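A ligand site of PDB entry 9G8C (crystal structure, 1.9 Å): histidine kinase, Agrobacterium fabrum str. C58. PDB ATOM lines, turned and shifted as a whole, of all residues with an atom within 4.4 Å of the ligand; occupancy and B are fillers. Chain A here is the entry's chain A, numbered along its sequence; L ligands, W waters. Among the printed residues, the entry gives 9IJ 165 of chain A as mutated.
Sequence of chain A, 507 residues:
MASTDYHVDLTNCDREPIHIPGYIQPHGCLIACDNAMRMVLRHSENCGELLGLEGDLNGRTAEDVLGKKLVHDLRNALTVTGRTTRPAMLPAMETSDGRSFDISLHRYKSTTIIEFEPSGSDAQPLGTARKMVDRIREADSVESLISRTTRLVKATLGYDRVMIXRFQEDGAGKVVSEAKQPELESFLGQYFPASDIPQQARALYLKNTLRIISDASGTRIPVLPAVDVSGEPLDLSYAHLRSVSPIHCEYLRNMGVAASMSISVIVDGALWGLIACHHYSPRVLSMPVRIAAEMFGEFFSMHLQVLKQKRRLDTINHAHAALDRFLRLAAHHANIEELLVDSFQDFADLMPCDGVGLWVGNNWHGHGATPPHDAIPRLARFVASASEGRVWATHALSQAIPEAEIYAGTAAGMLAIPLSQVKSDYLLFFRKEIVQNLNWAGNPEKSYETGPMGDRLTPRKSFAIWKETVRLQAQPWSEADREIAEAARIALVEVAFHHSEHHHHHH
C21 of the ligand is covalently linked to SG of Cys 13 (1.7 Å).
O of Asp 196 sits at hydrogen-bond distance from N1 of the ligand, at 3.0 Å.
OD2 of Asp 196 is in hydrogen-bond range of N4 of the ligand, 3.1 Å away.
A ring nitrogen (NE2) of His 278 sits at hydrogen-bond distance from an oxygen (O4) of the ligand (2.9 Å).
An oxygen (O3) of the ligand is in salt-bridge range of the guanidinium group (NH2) of Arg 211, at 3.0 Å.
An oxygen (O6) of the ligand lies close to the side-chain hydroxyl (OH) of Tyr 251 (3.1 Å).
The side-chain carboxylate (OD2) of Asp 196 is in hydrogen-bond range of the side-chain hydroxyl (OG) of Ser 462.
The guanidinium group of Arg 456 lies within salt-bridge range of the side-chain carboxylate of Asp 196 (2.7 Å).
NH1 of Arg 211 sits at hydrogen-bond distance from O of Arg 242 (2.9 Å).
The side-chain hydroxyl (OG) of Ser 462 is in hydrogen-bond range of the side-chain hydroxyl (OH) of Tyr 251, 2.7 Å away.
N of 9IJ 165 lies within hydrogen-bond range of O of Leu 274 (3.0 Å).
The backbone NH of Ile 247 lies within hydrogen-bond range of the side-chain hydroxyl of Ser 245 (3.0 Å).
The guanidinium group (NH2) of Arg 456 lies within hydrogen-bond range of the side-chain hydroxyl (OG) of Ser 195, at 3.2 Å.
The side-chain amide nitrogen of Gln 190 sits at hydrogen-bond distance from the backbone carbonyl oxygen of Pro 459 (3.2 Å).
Asp 14 touches the ligand.
9IJ 165 touches the ligand (CE2 to O2, 3.6 Å).
Phe 187 touches the ligand (CG to C24, 3.7 Å).
Gln 190 touches the ligand.
Phe 192 touches the ligand (CB to O6, 3.7 Å).
O of Ser 195 touches C5 of the ligand, at 3.9 Å.
CG1 of Ile 197 touches C7 of the ligand (3.8 Å).
CD of Pro 198 touches C27 of the ligand (3.3 Å).
CB of Ala 201 touches C18 of the ligand (3.9 Å).
Tyr 205 touches the ligand (OH to C23, 3.1 Å).
CD1 of Ile 213 touches O1 of the ligand, 3.8 Å away.
Ser 245 touches the ligand.
Ile 247 touches the ligand.
His 248 touches the ligand.
Ala 276 touches the ligand.
NH1 of Arg 456 touches O5 of the ligand, at 3.7 Å.
Leu 457 touches the ligand.
Pro 459 touches the ligand.
Ser 462 touches the ligand.
Hydrophobic or aromatic side chains that line the ligand: Phe 187, Phe 192, Ile 197, Pro 198, Ala 201, Ile 213, Ile 247, His 248, Tyr 251, Ala 276, His 278, Leu 457 and Pro 459.
Of the 30 residues printed, 24 come within 4 Å of the ligand.
Water W8 lies within hydrogen-bond range of an oxygen (O4) of the ligand and a ring nitrogen (NE2) of His 248.
Water W2 lies within hydrogen-bond range of an oxygen (O3) of the ligand (2.7 Å) and the backbone NH (N) of Ser 245 (2.8 Å).
Water W6 bridges O1 of the ligand (2.7 Å) and OH of Tyr 205 (2.8 Å).
Water W5 lies within hydrogen-bond range of an oxygen (O3) of the ligand and the guanidinium group (NH2) of Arg 242.
Water W7 bridges a ring nitrogen (ND1) of His 248 and a nitrogen (N1) of the ligand.
Water W4 lies within hydrogen-bond range of the side-chain amide nitrogen (NE2) of Gln 190 (2.7 Å), an oxygen (O6) of the ligand (2.8 Å) and the backbone carbonyl oxygen (O) of Pro 459 (3.3 Å).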
ATOM      1  N   LEU A  10      19.932  31.297   3.558  1.00  0.00           N
ATOM      2  CA  LEU A  10      19.735  29.830   3.630  1.00  0.00           C
ATOM      3  C   LEU A  10      20.642  29.115   2.626  1.00  0.00           C
ATOM      4  O   LEU A  10      20.866  27.896   2.795  1.00  0.00           O
ATOM      5  CB  LEU A  10      18.268  29.481   3.379  1.00  0.00           C
ATOM      6  CG  LEU A  10      17.290  30.090   4.374  1.00  0.00           C
ATOM      7  CD1 LEU A  10      15.876  29.583   4.124  1.00  0.00           C
ATOM      8  CD2 LEU A  10      17.713  29.809   5.811  1.00  0.00           C
ATOM      9  N   CYS A  13      24.409  29.602   4.748  1.00  0.00           N
ATOM     10  CA  CYS A  13      24.498  29.515   6.229  1.00  0.00           C
ATOM     11  C   CYS A  13      25.251  28.231   6.649  1.00  0.00           C
ATOM     12  O   CYS A  13      25.835  28.226   7.756  1.00  0.00           O
ATOM     13  CB  CYS A  13      23.136  29.674   6.881  1.00  0.00           C
ATOM     14  SG  CYS A  13      21.989  28.316   6.559  1.00  0.00           S
ATOM     15  N   ASP A  14      25.339  27.210   5.784  1.00  0.00           N
ATOM     16  CA  ASP A  14      26.114  25.972   6.111  1.00  0.00           C
ATOM     17  C   ASP A  14      27.602  26.282   6.282  1.00  0.00           C
ATOM     18  O   ASP A  14      28.308  25.443   6.886  1.00  0.00           O
ATOM     19  CB  ASP A  14      25.930  24.861   5.076  1.00  0.00           C
ATOM     20  CG  ASP A  14      26.374  25.210   3.661  1.00  0.00           C
ATOM     21  OD1 ASP A  14      26.507  26.410   3.365  1.00  0.00           O
ATOM     22  OD2 ASP A  14      26.588  24.280   2.877  1.00  0.00           O
ATOM     23  N   ILE A  18      31.195  31.968  11.558  1.00  0.00           N
ATOM     24  CA  ILE A  18      30.563  32.475  12.813  1.00  0.00           C
ATOM     25  C   ILE A  18      31.622  32.731  13.880  1.00  0.00           C
ATOM     26  O   ILE A  18      31.291  33.347  14.910  1.00  0.00           O
ATOM     27  CB  ILE A  18      29.465  31.509  13.312  1.00  0.00           C
ATOM     28  CG1 ILE A  18      29.995  30.085  13.482  1.00  0.00           C
ATOM     29  CG2 ILE A  18      28.256  31.586  12.388  1.00  0.00           C
ATOM     30  CD1 ILE A  18      29.026  29.147  14.166  1.00  0.00           C
ATOM     31  N   9IJ A 165      19.395  17.490  24.367  1.00  0.00           N
ATOM     32  CA  9IJ A 165      19.258  16.686  23.143  1.00  0.00           C
ATOM     33  C   9IJ A 165      20.464  15.794  22.906  1.00  0.00           C
ATOM     34  CB  9IJ A 165      18.918  17.539  21.902  1.00  0.00           C
ATOM     35  CG  9IJ A 165      19.931  18.562  21.491  1.00  0.00           C
ATOM     36  CD1 9IJ A 165      21.056  18.125  20.797  1.00  0.00           C
ATOM     37  CD2 9IJ A 165      19.746  19.923  21.728  1.00  0.00           C
ATOM     38  CE1 9IJ A 165      22.025  19.039  20.381  1.00  0.00           C
ATOM     39  CE2 9IJ A 165      20.709  20.823  21.296  1.00  0.00           C
ATOM     40  CZ  9IJ A 165      21.850  20.377  20.640  1.00  0.00           C
ATOM     41  C01 9IJ A 165      18.711  20.386  22.345  1.00  0.00           C
ATOM     42  N01 9IJ A 165      17.759  20.736  22.919  1.00  0.00           N
ATOM     43  O   9IJ A 165      21.670  16.342  23.367  1.00  0.00           O
ATOM     44  N   PHE A 187       8.675  20.128  23.102  1.00  0.00           N
ATOM     45  CA  PHE A 187       9.559  19.571  22.029  1.00  0.00           C
ATOM     46  C   PHE A 187      10.094  18.194  22.416  1.00  0.00           C
ATOM     47  O   PHE A 187      10.954  17.631  21.713  1.00  0.00           O
ATOM     48  CB  PHE A 187      10.716  20.537  21.749  1.00  0.00           C
ATOM     49  CG  PHE A 187      10.321  21.949  21.403  1.00  0.00           C
ATOM     50  CD1 PHE A 187       9.455  22.198  20.349  1.00  0.00           C
ATOM     51  CD2 PHE A 187      10.838  23.032  22.085  1.00  0.00           C
ATOM     52  CE1 PHE A 187       9.133  23.505  19.986  1.00  0.00           C
ATOM     53  CE2 PHE A 187      10.490  24.333  21.755  1.00  0.00           C
ATOM     54  CZ  PHE A 187       9.623  24.568  20.710  1.00  0.00           C
ATOM     55  N   GLN A 190      10.949  15.188  19.871  1.00  0.00           N
ATOM     56  CA  GLN A 190      11.141  15.833  18.540  1.00  0.00           C
ATOM     57  C   GLN A 190      12.597  15.668  18.100  1.00  0.00           C
ATOM     58  O   GLN A 190      13.474  15.552  18.974  1.00  0.00           O
ATOM     59  CB  GLN A 190      10.786  17.321  18.661  1.00  0.00           C
ATOM     60  CG  GLN A 190      10.682  18.036  17.333  1.00  0.00           C
ATOM     61  CD  GLN A 190       9.940  19.340  17.476  1.00  0.00           C
ATOM     62  OE1 GLN A 190       8.948  19.427  18.215  1.00  0.00           O
ATOM     63  NE2 GLN A 190      10.402  20.347  16.776  1.00  0.00           N
ATOM     64  N   PHE A 192      15.596  17.290  15.160  1.00  0.00           N
ATOM     65  CA  PHE A 192      15.963  18.304  14.138  1.00  0.00           C
ATOM     66  C   PHE A 192      17.075  17.725  13.283  1.00  0.00           C
ATOM     67  O   PHE A 192      17.885  16.924  13.763  1.00  0.00           O
ATOM     68  CB  PHE A 192      16.339  19.631  14.784  1.00  0.00           C
ATOM     69  CG  PHE A 192      17.442  19.559  15.812  1.00  0.00           C
ATOM     70  CD1 PHE A 192      18.777  19.561  15.421  1.00  0.00           C
ATOM     71  CD2 PHE A 192      17.154  19.564  17.167  1.00  0.00           C
ATOM     72  CE1 PHE A 192      19.788  19.537  16.355  1.00  0.00           C
ATOM     73  CE2 PHE A 192      18.171  19.536  18.108  1.00  0.00           C
ATOM     74  CZ  PHE A 192      19.486  19.543  17.707  1.00  0.00           C
ATOM     75  N   SER A 195      21.637  19.652   9.677  1.00  0.00           N
ATOM     76  CA  SER A 195      21.864  20.985   9.048  1.00  0.00           C
ATOM     77  C   SER A 195      21.416  22.142   9.963  1.00  0.00           C
ATOM     78  O   SER A 195      21.850  23.282   9.734  1.00  0.00           O
ATOM     79  CB  SER A 195      21.188  21.070   7.694  1.00  0.00           C
ATOM     80  OG  SER A 195      19.767  20.937   7.838  1.00  0.00           O
ATOM     81  N   ASP A 196      20.559  21.886  10.959  1.00  0.00           N
ATOM     82  CA  ASP A 196      20.114  22.948  11.908  1.00  0.00           C
ATOM     83  C   ASP A 196      21.288  23.435  12.757  1.00  0.00           C
ATOM     84  O   ASP A 196      21.184  24.541  13.343  1.00  0.00           O
ATOM     85  CB  ASP A 196      18.968  22.470  12.795  1.00  0.00           C
ATOM     86  CG  ASP A 196      17.615  22.583  12.138  1.00  0.00           C
ATOM     87  OD1 ASP A 196      17.562  22.775  10.891  1.00  0.00           O
ATOM     88  OD2 ASP A 196      16.622  22.462  12.868  1.00  0.00           O
ATOM     89  N   ILE A 197      22.362  22.643  12.836  1.00  0.00           N
ATOM     90  CA  ILE A 197      23.587  23.052  13.574  1.00  0.00           C
ATOM     91  C   ILE A 197      24.786  22.849  12.658  1.00  0.00           C
ATOM     92  O   ILE A 197      25.270  21.727  12.517  1.00  0.00           O
ATOM     93  CB  ILE A 197      23.746  22.335  14.927  1.00  0.00           C
ATOM     94  CG1 ILE A 197      22.484  22.483  15.797  1.00  0.00           C
ATOM     95  CG2 ILE A 197      24.980  22.858  15.659  1.00  0.00           C
ATOM     96  CD1 ILE A 197      22.574  21.752  17.115  1.00  0.00           C
ATOM     97  N   PRO A 198      25.268  23.931  12.008  1.00  0.00           N
ATOM     98  CA  PRO A 198      26.353  23.829  11.029  1.00  0.00           C
ATOM     99  C   PRO A 198      27.678  23.390  11.669  1.00  0.00           C
ATOM    100  O   PRO A 198      27.835  23.485  12.877  1.00  0.00           O
ATOM    101  CB  PRO A 198      26.435  25.239  10.406  1.00  0.00           C
ATOM    102  CG  PRO A 198      25.793  26.150  11.415  1.00  0.00           C
ATOM    103  CD  PRO A 198      24.737  25.300  12.105  1.00  0.00           C
ATOM    104  N   ALA A 201      29.576  25.628  14.072  1.00  0.00           N
ATOM    105  CA  ALA A 201      28.860  25.737  15.362  1.00  0.00           C
ATOM    106  C   ALA A 201      29.177  24.507  16.219  1.00  0.00           C
ATOM    107  O   ALA A 201      29.486  24.677  17.409  1.00  0.00           O
ATOM    108  CB  ALA A 201      27.377  25.915  15.157  1.00  0.00           C
ATOM    109  N   TYR A 205      30.977  24.376  19.904  1.00  0.00           N
ATOM    110  CA  TYR A 205      30.300  23.683  21.029  1.00  0.00           C
ATOM    111  C   TYR A 205      31.284  22.676  21.650  1.00  0.00           C
ATOM    112  O   TYR A 205      31.263  22.508  22.873  1.00  0.00           O
ATOM    113  CB  TYR A 205      28.987  23.006  20.606  1.00  0.00           C
ATOM    114  CG  TYR A 205      27.816  23.931  20.354  1.00  0.00           C
ATOM    115  CD1 TYR A 205      27.435  24.885  21.291  1.00  0.00           C
ATOM    116  CD2 TYR A 205      27.082  23.854  19.190  1.00  0.00           C
ATOM    117  CE1 TYR A 205      26.363  25.742  21.061  1.00  0.00           C
ATOM    118  CE2 TYR A 205      26.004  24.705  18.948  1.00  0.00           C
ATOM    119  CZ  TYR A 205      25.645  25.653  19.877  1.00  0.00           C
ATOM    120  OH  TYR A 205      24.567  26.478  19.622  1.00  0.00           O
ATOM    121  N   ARG A 211      27.878  28.272  25.874  1.00  0.00           N
ATOM    122  CA  ARG A 211      27.560  29.263  24.825  1.00  0.00           C
ATOM    123  C   ARG A 211      26.429  30.143  25.372  1.00  0.00           C
ATOM    124  O   ARG A 211      25.353  29.597  25.660  1.00  0.00           O
ATOM    125  CB  ARG A 211      27.206  28.571  23.518  1.00  0.00           C
ATOM    126  CG  ARG A 211      26.711  29.518  22.427  1.00  0.00           C
ATOM    127  CD  ARG A 211      27.717  30.618  22.174  1.00  0.00           C
ATOM    128  NE  ARG A 211      27.386  31.328  20.950  1.00  0.00           N
ATOM    129  CZ  ARG A 211      27.845  32.530  20.619  1.00  0.00           C
ATOM    130  NH1 ARG A 211      28.635  33.199  21.450  1.00  0.00           N
ATOM    131  NH2 ARG A 211      27.513  33.054  19.454  1.00  0.00           N
ATOM    132  N   ILE A 213      23.821  33.414  24.922  1.00  0.00           N
ATOM    133  CA  ILE A 213      23.082  34.424  24.111  1.00  0.00           C
ATOM    134  C   ILE A 213      22.242  35.247  25.100  1.00  0.00           C
ATOM    135  O   ILE A 213      21.199  34.733  25.545  1.00  0.00           O
ATOM    136  CB  ILE A 213      22.237  33.780  22.989  1.00  0.00           C
ATOM    137  CG1 ILE A 213      23.080  32.916  22.060  1.00  0.00           C
ATOM    138  CG2 ILE A 213      21.476  34.851  22.213  1.00  0.00           C
ATOM    139  CD1 ILE A 213      22.300  32.137  21.024  1.00  0.00           C
ATOM    140  N   ARG A 242      31.265  36.778  21.862  1.00  0.00           N
ATOM    141  CA  ARG A 242      31.117  36.569  20.391  1.00  0.00           C
ATOM    142  C   ARG A 242      29.629  36.667  20.009  1.00  0.00           C
ATOM    143  O   ARG A 242      28.806  35.969  20.637  1.00  0.00           O
ATOM    144  CB  ARG A 242      31.714  35.233  19.960  1.00  0.00           C
ATOM    145  CG  ARG A 242      31.577  34.945  18.467  1.00  0.00           C
ATOM    146  CD  ARG A 242      32.357  33.707  18.060  1.00  0.00           C
ATOM    147  NE  ARG A 242      31.947  32.580  18.907  1.00  0.00           N
ATOM    148  CZ  ARG A 242      30.916  31.789  18.680  1.00  0.00           C
ATOM    149  NH1 ARG A 242      30.191  31.937  17.583  1.00  0.00           N
ATOM    150  NH2 ARG A 242      30.623  30.823  19.539  1.00  0.00           N
ATOM    151  N   VAL A 244      26.073  36.457  17.556  1.00  0.00           N
ATOM    152  CA  VAL A 244      25.299  35.276  17.095  1.00  0.00           C
ATOM    153  C   VAL A 244      24.915  35.450  15.626  1.00  0.00           C
ATOM    154  O   VAL A 244      24.476  36.561  15.274  1.00  0.00           O
ATOM    155  CB  VAL A 244      24.042  35.083  17.955  1.00  0.00           C
ATOM    156  CG1 VAL A 244      23.377  33.744  17.672  1.00  0.00           C
ATOM    157  CG2 VAL A 244      24.314  35.249  19.441  1.00  0.00           C
ATOM    158  N   SER A 245      25.026  34.383  14.829  1.00  0.00           N
ATOM    159  CA  SER A 245      24.478  34.323  13.448  1.00  0.00           C
ATOM    160  C   SER A 245      23.102  34.948  13.396  1.00  0.00           C
ATOM    161  O   SER A 245      22.240  34.604  14.212  1.00  0.00           O
ATOM    162  CB  SER A 245      24.438  32.908  12.924  1.00  0.00           C
ATOM    163  OG  SER A 245      23.562  32.822  11.805  1.00  0.00           O
ATOM    164  N   ILE A 247      20.967  34.128  11.275  1.00  0.00           N
ATOM    165  CA  ILE A 247      20.128  32.929  10.986  1.00  0.00           C
ATOM    166  C   ILE A 247      19.582  32.420  12.321  1.00  0.00           C
ATOM    167  O   ILE A 247      18.347  32.268  12.453  1.00  0.00           O
ATOM    168  CB  ILE A 247      20.920  31.846  10.227  1.00  0.00           C
ATOM    169  CG1 ILE A 247      21.474  32.393   8.904  1.00  0.00           C
ATOM    170  CG2 ILE A 247      20.084  30.588   9.988  1.00  0.00           C
ATOM    171  CD1 ILE A 247      20.424  32.946   7.965  1.00  0.00           C
ATOM    172  N   HIS A 248      20.457  32.166  13.294  1.00  0.00           N
ATOM    173  CA  HIS A 248      20.019  31.614  14.601  1.00  0.00           C
ATOM    174  C   HIS A 248      19.154  32.643  15.337  1.00  0.00           C
ATOM    175  O   HIS A 248      18.181  32.224  15.969  1.00  0.00           O
ATOM    176  CB  HIS A 248      21.183  31.104  15.451  1.00  0.00           C
ATOM    177  CG  HIS A 248      20.720  30.363  16.668  1.00  0.00           C
ATOM    178  ND1 HIS A 248      19.899  29.254  16.578  1.00  0.00           N
ATOM    179  CD2 HIS A 248      20.918  30.595  17.982  1.00  0.00           C
ATOM    180  CE1 HIS A 248      19.637  28.813  17.794  1.00  0.00           C
ATOM    181  NE2 HIS A 248      20.259  29.614  18.679  1.00  0.00           N
ATOM    182  N   TYR A 251      15.700  32.368  13.987  1.00  0.00           N
ATOM    183  CA  TYR A 251      15.135  31.089  14.494  1.00  0.00           C
ATOM    184  C   TYR A 251      14.585  31.325  15.907  1.00  0.00           C
ATOM    185  O   TYR A 251      13.387  31.010  16.163  1.00  0.00           O
ATOM    186  CB  TYR A 251      16.175  29.954  14.412  1.00  0.00           C
ATOM    187  CG  TYR A 251      15.555  28.568  14.376  1.00  0.00           C
ATOM    188  CD1 TYR A 251      14.856  28.096  15.465  1.00  0.00           C
ATOM    189  CD2 TYR A 251      15.660  27.750  13.264  1.00  0.00           C
ATOM    190  CE1 TYR A 251      14.263  26.850  15.464  1.00  0.00           C
ATOM    191  CE2 TYR A 251      15.075  26.489  13.248  1.00  0.00           C
ATOM    192  CZ  TYR A 251      14.376  26.034  14.346  1.00  0.00           C
ATOM    193  OH  TYR A 251      13.782  24.799  14.366  1.00  0.00           O
ATOM    194  N   MET A 255      10.620  31.436  17.474  1.00  0.00           N
ATOM    195  CA  MET A 255      10.166  30.579  18.609  1.00  0.00           C
ATOM    196  C   MET A 255       9.571  31.447  19.724  1.00  0.00           C
ATOM    197  O   MET A 255       8.743  30.929  20.505  1.00  0.00           O
ATOM    198  CB  MET A 255      11.336  29.766  19.173  1.00  0.00           C
ATOM    199  CG  MET A 255      11.845  28.702  18.226  1.00  0.00           C
ATOM    200  SD  MET A 255      13.312  27.895  18.881  1.00  0.00           S
ATOM    201  CE  MET A 255      12.596  26.989  20.253  1.00  0.00           C
ATOM    202  N   LEU A 274      23.804  18.692  23.874  1.00  0.00           N
ATOM    203  CA  LEU A 274      23.802  19.903  24.737  1.00  0.00           C
ATOM    204  C   LEU A 274      22.717  19.779  25.811  1.00  0.00           C
ATOM    205  O   LEU A 274      21.655  19.161  25.530  1.00  0.00           O
ATOM    206  CB  LEU A 274      23.533  21.162  23.911  1.00  0.00           C
ATOM    207  CG  LEU A 274      24.478  21.447  22.743  1.00  0.00           C
ATOM    208  CD1 LEU A 274      24.042  22.710  22.003  1.00  0.00           C
ATOM    209  CD2 LEU A 274      25.923  21.585  23.213  1.00  0.00           C
ATOM    210  N   ALA A 276      20.459  22.595  26.811  1.00  0.00           N
ATOM    211  CA  ALA A 276      20.040  23.862  26.172  1.00  0.00           C
ATOM    212  C   ALA A 276      19.059  24.597  27.094  1.00  0.00           C
ATOM    213  O   ALA A 276      17.968  24.047  27.323  1.00  0.00           O
ATOM    214  CB  ALA A 276      19.427  23.573  24.826  1.00  0.00           C
ATOM    215  N   HIS A 278      16.757  27.912  27.547  1.00  0.00           N
ATOM    216  CA  HIS A 278      16.048  28.945  26.736  1.00  0.00           C
ATOM    217  C   HIS A 278      15.210  29.814  27.677  1.00  0.00           C
ATOM    218  O   HIS A 278      14.556  29.253  28.585  1.00  0.00           O
ATOM    219  CB  HIS A 278      15.175  28.298  25.664  1.00  0.00           C
ATOM    220  CG  HIS A 278      15.891  27.621  24.545  1.00  0.00           C
ATOM    221  ND1 HIS A 278      15.206  27.084  23.470  1.00  0.00           N
ATOM    222  CD2 HIS A 278      17.206  27.414  24.301  1.00  0.00           C
ATOM    223  CE1 HIS A 278      16.071  26.549  22.622  1.00  0.00           C
ATOM    224  NE2 HIS A 278      17.305  26.759  23.109  1.00  0.00           N
ATOM    225  N   ARG A 456      11.595  27.995   6.938  1.00  0.00           N
ATOM    226  CA  ARG A 456      12.777  27.137   7.257  1.00  0.00           C
ATOM    227  C   ARG A 456      13.128  27.240   8.756  1.00  0.00           C
ATOM    228  O   ARG A 456      13.502  26.208   9.330  1.00  0.00           O
ATOM    229  CB  ARG A 456      13.976  27.492   6.390  1.00  0.00           C
ATOM    230  CG  ARG A 456      15.239  26.709   6.736  1.00  0.00           C
ATOM    231  CD  ARG A 456      15.047  25.203   6.573  1.00  0.00           C
ATOM    232  NE  ARG A 456      16.249  24.459   6.865  1.00  0.00           N
ATOM    233  CZ  ARG A 456      16.609  23.996   8.065  1.00  0.00           C
ATOM    234  NH1 ARG A 456      15.831  24.217   9.114  1.00  0.00           N
ATOM    235  NH2 ARG A 456      17.721  23.330   8.206  1.00  0.00           N
ATOM    236  N   LEU A 457      13.043  28.429   9.355  1.00  0.00           N
ATOM    237  CA  LEU A 457      13.647  28.697  10.697  1.00  0.00           C
ATOM    238  C   LEU A 457      12.560  28.558  11.779  1.00  0.00           C
ATOM    239  O   LEU A 457      12.387  29.487  12.585  1.00  0.00           O
ATOM    240  CB  LEU A 457      14.301  30.082  10.690  1.00  0.00           C
ATOM    241  CG  LEU A 457      15.324  30.342   9.570  1.00  0.00           C
ATOM    242  CD1 LEU A 457      15.868  31.758   9.657  1.00  0.00           C
ATOM    243  CD2 LEU A 457      16.482  29.348   9.602  1.00  0.00           C
ATOM    244  N   PRO A 459      10.661  25.313  14.489  1.00  0.00           N
ATOM    245  CA  PRO A 459      10.681  23.914  14.934  1.00  0.00           C
ATOM    246  C   PRO A 459       9.770  22.983  14.113  1.00  0.00           C
ATOM    247  O   PRO A 459      10.136  21.829  13.928  1.00  0.00           O
ATOM    248  CB  PRO A 459      10.236  24.029  16.406  1.00  0.00           C
ATOM    249  CG  PRO A 459      10.680  25.412  16.828  1.00  0.00           C
ATOM    250  CD  PRO A 459      10.446  26.260  15.593  1.00  0.00           C
ATOM    251  N   SER A 462      11.770  22.328  10.829  1.00  0.00           N
ATOM    252  CA  SER A 462      12.925  21.485  11.208  1.00  0.00           C
ATOM    253  C   SER A 462      12.489  20.020  11.370  1.00  0.00           C
ATOM    254  O   SER A 462      13.150  19.118  10.856  1.00  0.00           O
ATOM    255  CB  SER A 462      13.592  21.990  12.479  1.00  0.00           C
ATOM    256  OG  SER A 462      14.301  23.216  12.273  1.00  0.00           O
HETATM  257  C1  LIG L   1      19.247  26.582  11.049  1.00  0.00           C
HETATM  258  C2  LIG L   1      22.750  27.823  13.458  1.00  0.00           C
HETATM  259  O1  LIG L   1      25.113  30.086  19.513  1.00  0.00           O
HETATM  260  C3  LIG L   1      21.178  25.851  17.012  1.00  0.00           C
HETATM  261  O2  LIG L   1      20.102  24.318  21.552  1.00  0.00           O
HETATM  262  C4  LIG L   1      16.810  23.924  16.677  1.00  0.00           C
HETATM  263  C5  LIG L   1      19.971  26.647   9.856  1.00  0.00           C
HETATM  264  C6  LIG L   1      23.866  28.385  14.072  1.00  0.00           C
HETATM  265  O3  LIG L   1      26.279  30.928  17.813  1.00  0.00           O
HETATM  266  C7  LIG L   1      20.908  25.036  18.126  1.00  0.00           C
HETATM  267  O4  LIG L   1      19.968  26.475  22.029  1.00  0.00           O
HETATM  268  C8  LIG L   1      16.120  24.189  17.857  1.00  0.00           C
HETATM  269  C9  LIG L   1      21.257  27.143  10.040  1.00  0.00           C
HETATM  270  C10 LIG L   1      23.810  28.061  15.427  1.00  0.00           C
HETATM  271  C11 LIG L   1      19.748  24.349  17.850  1.00  0.00           C
HETATM  272  C12 LIG L   1      14.908  23.500  17.764  1.00  0.00           C
HETATM  273  C13 LIG L   1      21.350  27.323  11.416  1.00  0.00           C
HETATM  274  C14 LIG L   1      22.708  27.228  15.575  1.00  0.00           C
HETATM  275  C15 LIG L   1      19.202  24.849  16.671  1.00  0.00           C
HETATM  276  C16 LIG L   1      14.841  22.855  16.535  1.00  0.00           C
HETATM  277  C17 LIG L   1      22.259  27.350   9.050  1.00  0.00           C
HETATM  278  C18 LIG L   1      24.751  28.498  16.517  1.00  0.00           C
HETATM  279  C19 LIG L   1      21.770  24.818  19.338  1.00  0.00           C
HETATM  280  C20 LIG L   1      13.926  23.489  18.767  1.00  0.00           C
HETATM  281  C21 LIG L   1      22.177  27.096   7.711  1.00  0.00           C
HETATM  282  C22 LIG L   1      24.278  29.705  17.310  1.00  0.00           C
HETATM  283  C23 LIG L   1      21.621  25.824  20.458  1.00  0.00           C
HETATM  284  C24 LIG L   1      12.838  22.739  18.792  1.00  0.00           C
HETATM  285  C25 LIG L   1      25.308  30.269  18.278  1.00  0.00           C
HETATM  286  C26 LIG L   1      20.474  25.508  21.402  1.00  0.00           C
HETATM  287  C27 LIG L   1      22.478  27.770  12.102  1.00  0.00           C
HETATM  288  C28 LIG L   1      22.248  26.710  16.792  1.00  0.00           C
HETATM  289  C29 LIG L   1      18.054  24.259  16.182  1.00  0.00           C
HETATM  290  C30 LIG L   1      19.262  26.845   8.547  1.00  0.00           C
HETATM  291  C31 LIG L   1      24.922  29.248  13.444  1.00  0.00           C
HETATM  292  C32 LIG L   1      19.131  23.320  18.753  1.00  0.00           C
HETATM  293  C33 LIG L   1      16.557  25.052  19.000  1.00  0.00           C
HETATM  294  N1  LIG L   1      20.126  27.035  12.018  1.00  0.00           N
HETATM  295  O5  LIG L   1      18.087  26.286  11.242  1.00  0.00           O
HETATM  296  N2  LIG L   1      22.085  27.044  14.376  1.00  0.00           N
HETATM  297  N3  LIG L   1      20.160  25.657  16.111  1.00  0.00           N
HETATM  298  N4  LIG L   1      16.001  23.140  15.874  1.00  0.00           N
HETATM  299  O6  LIG L   1      13.958  22.155  16.034  1.00  0.00           O
HETATM  300  O   HOH W   1      25.608  29.302  10.185  1.00  0.00           O
HETATM  301  O   HOH W   2      26.660  32.149  15.467  1.00  0.00           O
HETATM  302  O   HOH W   3      21.041  26.934  24.606  1.00  0.00           O
HETATM  303  O   HOH W   4      12.511  19.882  15.157  1.00  0.00           O
HETATM  304  O   HOH W   5      28.658  29.590  17.989  1.00  0.00           O
HETATM  305  O   HOH W   6      23.609  28.616  21.203  1.00  0.00           O
HETATM  306  O   HOH W   7      18.983  27.711  14.506  1.00  0.00           O
HETATM  307  O   HOH W   8      20.816  28.849  21.342  1.00  0.00           O
